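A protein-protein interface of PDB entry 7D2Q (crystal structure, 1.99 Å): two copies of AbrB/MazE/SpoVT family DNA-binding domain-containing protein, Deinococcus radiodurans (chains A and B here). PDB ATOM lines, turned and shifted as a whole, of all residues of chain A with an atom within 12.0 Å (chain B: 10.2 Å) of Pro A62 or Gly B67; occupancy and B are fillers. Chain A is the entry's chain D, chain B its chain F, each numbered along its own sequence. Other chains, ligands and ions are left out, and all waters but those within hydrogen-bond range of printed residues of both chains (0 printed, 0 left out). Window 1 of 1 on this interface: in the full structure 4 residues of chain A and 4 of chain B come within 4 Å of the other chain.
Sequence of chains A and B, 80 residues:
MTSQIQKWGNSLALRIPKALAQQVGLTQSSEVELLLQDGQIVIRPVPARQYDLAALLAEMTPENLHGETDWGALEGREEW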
ATOM      1  N   LEU A  56       7.265 -24.761  -4.253  1.00  0.00           N
ATOM      2  CA  LEU A  56       7.940 -23.468  -4.355  1.00  0.00           C
ATOM      3  C   LEU A  56       8.129 -22.829  -2.985  1.00  0.00           C
ATOM      4  O   LEU A  56       9.237 -22.410  -2.637  1.00  0.00           O
ATOM      5  CB  LEU A  56       7.148 -22.520  -5.266  1.00  0.00           C
ATOM      6  CG  LEU A  56       7.092 -22.826  -6.763  1.00  0.00           C
ATOM      7  CD1 LEU A  56       6.064 -21.927  -7.421  1.00  0.00           C
ATOM      8  CD2 LEU A  56       8.461 -22.656  -7.421  1.00  0.00           C
ATOM      9  N   LEU A  57       7.050 -22.710  -2.200  1.00  0.00           N
ATOM     10  CA  LEU A  57       7.174 -21.983  -0.942  1.00  0.00           C
ATOM     11  C   LEU A  57       8.086 -22.706   0.043  1.00  0.00           C
ATOM     12  O   LEU A  57       8.796 -22.051   0.813  1.00  0.00           O
ATOM     13  CB  LEU A  57       5.802 -21.737  -0.315  1.00  0.00           C
ATOM     14  CG  LEU A  57       4.789 -20.878  -1.077  1.00  0.00           C
ATOM     15  CD1 LEU A  57       3.572 -20.580  -0.204  1.00  0.00           C
ATOM     16  CD2 LEU A  57       5.403 -19.568  -1.587  1.00  0.00           C
ATOM     17  N   ALA A  58       8.110 -24.044   0.022  1.00  0.00           N
ATOM     18  CA  ALA A  58       8.997 -24.770   0.928  1.00  0.00           C
ATOM     19  C   ALA A  58      10.465 -24.513   0.627  1.00  0.00           C
ATOM     20  O   ALA A  58      11.308 -24.741   1.497  1.00  0.00           O
ATOM     21  CB  ALA A  58       8.728 -26.277   0.873  1.00  0.00           C
ATOM     22  N   GLU A  59      10.795 -24.040  -0.574  1.00  0.00           N
ATOM     23  CA  GLU A  59      12.193 -23.766  -0.872  1.00  0.00           C
ATOM     24  C   GLU A  59      12.638 -22.378  -0.417  1.00  0.00           C
ATOM     25  O   GLU A  59      13.843 -22.111  -0.426  1.00  0.00           O
ATOM     26  CB  GLU A  59      12.455 -23.950  -2.372  1.00  0.00           C
ATOM     27  CG  GLU A  59      12.474 -25.416  -2.820  1.00  0.00           C
ATOM     28  CD  GLU A  59      12.294 -25.591  -4.327  1.00  0.00           C
ATOM     29  OE1 GLU A  59      12.867 -24.788  -5.100  1.00  0.00           O
ATOM     30  OE2 GLU A  59      11.578 -26.538  -4.739  1.00  0.00           O
ATOM     31  N   MET A  60      11.716 -21.505  -0.004  1.00  0.00           N
ATOM     32  CA  MET A  60      12.069 -20.183   0.518  1.00  0.00           C
ATOM     33  C   MET A  60      12.622 -20.297   1.930  1.00  0.00           C
ATOM     34  O   MET A  60      12.035 -20.970   2.784  1.00  0.00           O
ATOM     35  CB  MET A  60      10.850 -19.256   0.536  1.00  0.00           C
ATOM     36  CG  MET A  60      10.145 -19.100  -0.797  1.00  0.00           C
ATOM     37  SD  MET A  60       9.021 -17.680  -0.782  1.00  0.00           S
ATOM     38  CE  MET A  60       8.010 -18.127   0.616  1.00  0.00           C
ATOM     39  N   THR A  61      13.748 -19.645   2.174  1.00  0.00           N
ATOM     40  CA  THR A  61      14.349 -19.561   3.494  1.00  0.00           C
ATOM     41  C   THR A  61      14.789 -18.131   3.761  1.00  0.00           C
ATOM     42  O   THR A  61      14.994 -17.350   2.822  1.00  0.00           O
ATOM     43  CB  THR A  61      15.576 -20.474   3.619  1.00  0.00           C
ATOM     44  OG1 THR A  61      16.651 -19.852   2.923  1.00  0.00           O
ATOM     45  CG2 THR A  61      15.316 -21.860   3.016  1.00  0.00           C
ATOM     46  N   PRO A  62      14.987 -17.764   5.030  1.00  0.00           N
ATOM     47  CA  PRO A  62      15.537 -16.435   5.323  1.00  0.00           C
ATOM     48  C   PRO A  62      16.887 -16.185   4.676  1.00  0.00           C
ATOM     49  O   PRO A  62      17.299 -15.027   4.567  1.00  0.00           O
ATOM     50  CB  PRO A  62      15.629 -16.424   6.854  1.00  0.00           C
ATOM     51  CG  PRO A  62      14.541 -17.354   7.286  1.00  0.00           C
ATOM     52  CD  PRO A  62      14.533 -18.450   6.256  1.00  0.00           C
ATOM     53  N   GLU A  63      17.572 -17.218   4.207  1.00  0.00           N
ATOM     54  CA  GLU A  63      18.875 -17.041   3.587  1.00  0.00           C
ATOM     55  C   GLU A  63      18.797 -16.760   2.083  1.00  0.00           C
ATOM     56  O   GLU A  63      19.786 -16.317   1.502  1.00  0.00           O
ATOM     57  CB  GLU A  63      19.739 -18.282   3.847  1.00  0.00           C
ATOM     58  CG  GLU A  63      20.140 -18.489   5.325  1.00  0.00           C
ATOM     59  CD  GLU A  63      18.960 -18.844   6.216  1.00  0.00           C
ATOM     60  OE1 GLU A  63      18.263 -19.844   5.942  1.00  0.00           O
ATOM     61  OE2 GLU A  63      18.700 -18.099   7.179  1.00  0.00           O
ATOM     62  N   ASN A  64      17.657 -16.990   1.430  1.00  0.00           N
ATOM     63  CA  ASN A  64      17.575 -16.739  -0.008  1.00  0.00           C
ATOM     64  C   ASN A  64      16.484 -15.740  -0.410  1.00  0.00           C
ATOM     65  O   ASN A  64      16.187 -15.622  -1.601  1.00  0.00           O
ATOM     66  CB  ASN A  64      17.414 -18.060  -0.775  1.00  0.00           C
ATOM     67  CG  ASN A  64      16.105 -18.798  -0.455  1.00  0.00           C
ATOM     68  OD1 ASN A  64      15.131 -18.204  -0.023  1.00  0.00           O
ATOM     69  ND2 ASN A  64      16.086 -20.110  -0.701  1.00  0.00           N
ATOM     70  N   LEU A  65      15.896 -15.004   0.530  1.00  0.00           N
ATOM     71  CA  LEU A  65      14.880 -14.008   0.181  1.00  0.00           C
ATOM     72  C   LEU A  65      15.476 -12.828  -0.604  1.00  0.00           C
ATOM     73  O   LEU A  65      16.665 -12.519  -0.509  1.00  0.00           O
ATOM     74  CB  LEU A  65      14.210 -13.487   1.449  1.00  0.00           C
ATOM     75  CG  LEU A  65      13.572 -14.531   2.360  1.00  0.00           C
ATOM     76  CD1 LEU A  65      12.823 -13.856   3.492  1.00  0.00           C
ATOM     77  CD2 LEU A  65      12.643 -15.448   1.554  1.00  0.00           C
ATOM     78  N   HIS A  66      14.617 -12.149  -1.372  1.00  0.00           N
ATOM     79  CA  HIS A  66      14.919 -10.857  -1.988  1.00  0.00           C
ATOM     80  C   HIS A  66      13.851  -9.850  -1.565  1.00  0.00           C
ATOM     81  O   HIS A  66      12.657 -10.079  -1.786  1.00  0.00           O
ATOM     82  CB  HIS A  66      14.935 -10.932  -3.521  1.00  0.00           C
ATOM     83  CG  HIS A  66      15.878 -11.945  -4.092  1.00  0.00           C
ATOM     84  ND1 HIS A  66      17.091 -11.601  -4.652  1.00  0.00           N
ATOM     85  CD2 HIS A  66      15.764 -13.287  -4.239  1.00  0.00           C
ATOM     86  CE1 HIS A  66      17.691 -12.688  -5.105  1.00  0.00           C
ATOM     87  NE2 HIS A  66      16.910 -13.725  -4.862  1.00  0.00           N
ATOM     88  N   GLY A  67      14.270  -8.724  -1.012  1.00  0.00           N
ATOM     89  CA  GLY A  67      13.336  -7.683  -0.623  1.00  0.00           C
ATOM     90  C   GLY A  67      12.710  -7.009  -1.831  1.00  0.00           C
ATOM     91  O   GLY A  67      12.997  -7.328  -2.986  1.00  0.00           O
ATOM     92  N   THR B  61      13.189  -4.086   7.736  1.00  0.00           N
ATOM     93  CA  THR B  61      12.326  -4.214   6.575  1.00  0.00           C
ATOM     94  C   THR B  61      12.801  -5.415   5.777  1.00  0.00           C
ATOM     95  O   THR B  61      13.966  -5.813   5.879  1.00  0.00           O
ATOM     96  CB  THR B  61      12.363  -2.964   5.678  1.00  0.00           C
ATOM     97  OG1 THR B  61      13.597  -2.941   4.961  1.00  0.00           O
ATOM     98  CG2 THR B  61      12.214  -1.668   6.483  1.00  0.00           C
ATOM     99  N   PRO B  62      11.936  -5.997   4.946  1.00  0.00           N
ATOM    100  CA  PRO B  62      12.397  -7.041   4.020  1.00  0.00           C
ATOM    101  C   PRO B  62      13.569  -6.613   3.154  1.00  0.00           C
ATOM    102  O   PRO B  62      14.231  -7.482   2.579  1.00  0.00           O
ATOM    103  CB  PRO B  62      11.151  -7.327   3.169  1.00  0.00           C
ATOM    104  CG  PRO B  62      10.018  -7.025   4.089  1.00  0.00           C
ATOM    105  CD  PRO B  62      10.464  -5.869   4.950  1.00  0.00           C
ATOM    106  N   GLU B  63      13.875  -5.319   3.077  1.00  0.00           N
ATOM    107  CA  GLU B  63      14.942  -4.825   2.222  1.00  0.00           C
ATOM    108  C   GLU B  63      16.286  -4.728   2.931  1.00  0.00           C
ATOM    109  O   GLU B  63      17.302  -4.519   2.261  1.00  0.00           O
ATOM    110  CB  GLU B  63      14.574  -3.447   1.644  1.00  0.00           C
ATOM    111  CG  GLU B  63      13.472  -3.508   0.581  1.00  0.00           C
ATOM    112  CD  GLU B  63      12.109  -3.756   1.194  1.00  0.00           C
ATOM    113  OE1 GLU B  63      11.690  -2.925   2.026  1.00  0.00           O
ATOM    114  OE2 GLU B  63      11.467  -4.786   0.871  1.00  0.00           O
ATOM    115  N   ASN B  64      16.337  -4.897   4.254  1.00  0.00           N
ATOM    116  CA  ASN B  64      17.618  -4.816   4.942  1.00  0.00           C
ATOM    117  C   ASN B  64      17.910  -6.028   5.822  1.00  0.00           C
ATOM    118  O   ASN B  64      18.839  -5.967   6.624  1.00  0.00           O
ATOM    119  CB  ASN B  64      17.721  -3.507   5.765  1.00  0.00           C
ATOM    120  CG  ASN B  64      16.686  -3.403   6.892  1.00  0.00           C
ATOM    121  OD1 ASN B  64      16.141  -4.400   7.359  1.00  0.00           O
ATOM    122  ND2 ASN B  64      16.432  -2.174   7.342  1.00  0.00           N
ATOM    123  N   LEU B  65      17.167  -7.126   5.677  1.00  0.00           N
ATOM    124  CA  LEU B  65      17.382  -8.303   6.506  1.00  0.00           C
ATOM    125  C   LEU B  65      18.701  -8.997   6.165  1.00  0.00           C
ATOM    126  O   LEU B  65      19.206  -8.916   5.044  1.00  0.00           O
ATOM    127  CB  LEU B  65      16.225  -9.299   6.346  1.00  0.00           C
ATOM    128  CG  LEU B  65      14.829  -8.774   6.672  1.00  0.00           C
ATOM    129  CD1 LEU B  65      13.806  -9.891   6.592  1.00  0.00           C
ATOM    130  CD2 LEU B  65      14.800  -8.076   8.040  1.00  0.00           C
ATOM    131  N   HIS B  66      19.257  -9.683   7.159  1.00  0.00           N
ATOM    132  CA  HIS B  66      20.433 -10.534   7.002  1.00  0.00           C
ATOM    133  C   HIS B  66      20.048 -11.942   7.440  1.00  0.00           C
ATOM    134  O   HIS B  66      19.746 -12.154   8.616  1.00  0.00           O
ATOM    135  CB  HIS B  66      21.604 -10.052   7.861  1.00  0.00           C
ATOM    136  CG  HIS B  66      22.155  -8.713   7.477  1.00  0.00           C
ATOM    137  ND1 HIS B  66      23.269  -8.572   6.679  1.00  0.00           N
ATOM    138  CD2 HIS B  66      21.778  -7.458   7.825  1.00  0.00           C
ATOM    139  CE1 HIS B  66      23.545  -7.287   6.538  1.00  0.00           C
ATOM    140  NE2 HIS B  66      22.654  -6.590   7.221  1.00  0.00           N
ATOM    141  N   GLY B  67      20.101 -12.903   6.524  1.00  0.00           N
ATOM    142  CA  GLY B  67      19.789 -14.282   6.860  1.00  0.00           C
ATOM    143  C   GLY B  67      20.813 -14.900   7.809  1.00  0.00           C
ATOM    144  O   GLY B  67      21.814 -14.291   8.188  1.00  0.00           O
ATOM    145  N   GLU B  68      20.549 -16.154   8.184  1.00  0.00           N
ATOM    146  CA  GLU B  68      21.400 -16.858   9.141  1.00  0.00           C
ATOM    147  C   GLU B  68      22.829 -16.952   8.617  1.00  0.00           C
ATOM    148  O   GLU B  68      23.059 -17.296   7.457  1.00  0.00           O
ATOM    149  CB  GLU B  68      20.841 -18.262   9.428  1.00  0.00           C
ATOM    150  CG  GLU B  68      21.480 -18.989  10.634  1.00  0.00           C
ATOM    151  CD  GLU B  68      21.256 -20.518  10.627  1.00  0.00           C
ATOM    152  OE1 GLU B  68      22.254 -21.269  10.498  1.00  0.00           O
ATOM    153  OE2 GLU B  68      20.092 -20.971  10.752  1.00  0.00           O
ATOM    154  N   THR B  69      23.786 -16.625   9.478  1.00  0.00           N
ATOM    155  CA  THR B  69      25.193 -16.688   9.112  1.00  0.00           C
ATOM    156  C   THR B  69      25.614 -18.133   8.897  1.00  0.00           C
ATOM    157  O   THR B  69      25.340 -19.000   9.731  1.00  0.00           O
ATOM    158  CB  THR B  69      26.044 -16.067  10.216  1.00  0.00           C
ATOM    159  OG1 THR B  69      25.675 -14.693  10.372  1.00  0.00           O
ATOM    160  CG2 THR B  69      27.529 -16.190   9.878  1.00  0.00           C
ATOM    161  N   ASP B  70      26.283 -18.394   7.779  1.00  0.00           N
ATOM    162  CA  ASP B  70      26.725 -19.751   7.478  1.00  0.00           C
ATOM    163  C   ASP B  70      28.015 -20.032   8.232  1.00  0.00           C
ATOM    164  O   ASP B  70      29.079 -19.525   7.864  1.00  0.00           O
ATOM    165  CB  ASP B  70      26.934 -19.944   5.978  1.00  0.00           C
ATOM    166  CG  ASP B  70      27.422 -21.350   5.638  1.00  0.00           C
ATOM    167  OD1 ASP B  70      27.087 -22.295   6.391  1.00  0.00           O
ATOM    168  OD2 ASP B  70      28.143 -21.504   4.625  1.00  0.00           O
ATOM    169  N   TRP B  71      27.931 -20.848   9.280  1.00  0.00           N
ATOM    170  CA  TRP B  71      29.119 -21.331   9.962  1.00  0.00           C
ATOM    171  C   TRP B  71      29.465 -22.754   9.557  1.00  0.00           C
ATOM    172  O   TRP B  71      30.276 -23.403  10.224  1.00  0.00           O
ATOM    173  CB  TRP B  71      28.932 -21.225  11.474  1.00  0.00           C
ATOM    174  CG  TRP B  71      29.004 -19.810  11.951  1.00  0.00           C
ATOM    175  CD1 TRP B  71      27.962 -19.026  12.382  1.00  0.00           C
ATOM    176  CD2 TRP B  71      30.173 -18.997  12.015  1.00  0.00           C
ATOM    177  NE1 TRP B  71      28.429 -17.776  12.732  1.00  0.00           N
ATOM    178  CE2 TRP B  71      29.781 -17.734  12.511  1.00  0.00           C
ATOM    179  CE3 TRP B  71      31.520 -19.213  11.701  1.00  0.00           C
ATOM    180  CZ2 TRP B  71      30.690 -16.696  12.716  1.00  0.00           C
ATOM    181  CZ3 TRP B  71      32.424 -18.173  11.901  1.00  0.00           C
ATOM    182  CH2 TRP B  71      32.001 -16.932  12.406  1.00  0.00           C
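Of the 11 printed residues of chain B, 4 touch a printed residue of chain A. Printed residues of chain B that touch a printed residue of chain A: Pro B62, Glu B63, Gly B67 and Glu B68. Along chain B the printed residues that touch a printed residue of chain A span positions 62 to 68.
The backbone NH of Glu B68 is in hydrogen-bond range of the side-chain carboxylate of Glu A63, at 2.9 Å.
The side-chain hydroxyl (OG1) of Thr A61 lies close to the backbone NH (N) of Glu A63 (3.1 Å). The side-chain hydroxyl of Thr B61 sits close to the backbone NH of Glu B63 (3.0 Å).
Pro A62 touches Gly B67, and with the chains exchanged Gly A67 touches Pro B62. Glu A63 touches Gly B67, and with the chains exchanged Gly A67 touches Glu B63. Of the 5 pairs that touch across the chains among the printed residues, 4 have their exchanged pair printed and touching as well.
Pro A62 touches Gly B67 (O to CA, 3.5 Å). Gly B67 touches Glu A63. Gly A67 touches Pro B62. Gly A67 touches Glu B63.
Of the printed residues of chain B, Pro A62 touches Gly B67. Of chain A, only Pro A62 (3.5 Å) and Glu A63 (3.9 Å) come within 4 Å of Gly B67. No residue of chain B comes within 4 Å of Thr A61. Of chain B, only Gly B67 (3.9 Å) and Glu B68 (2.9 Å) come within 4 Å of Glu A63. No residue of chain A comes within 4 Å of Leu B65. No residue of chain A comes within 4 Å of His B66. Glu B68 touches just one residue of chain A: Glu A63. No residue of chain A comes within 4 Å of Thr B69. Of the printed residues of chain A, Glu B63 touches Gly A67 (3.7 Å). Of the printed residues of chain A, Pro B62 touches Gly A67. Of the printed residues of chain B, Gly A67 touches Pro B62 (3.3 Å) and Glu B63 (3.7 Å). Asn B64 touches none of the printed residues of chain A. His A66 touches none of the printed residues of chain B. The nearest residue of chain B that does not touch Pro A62 is Glu B68 (5.0 Å).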
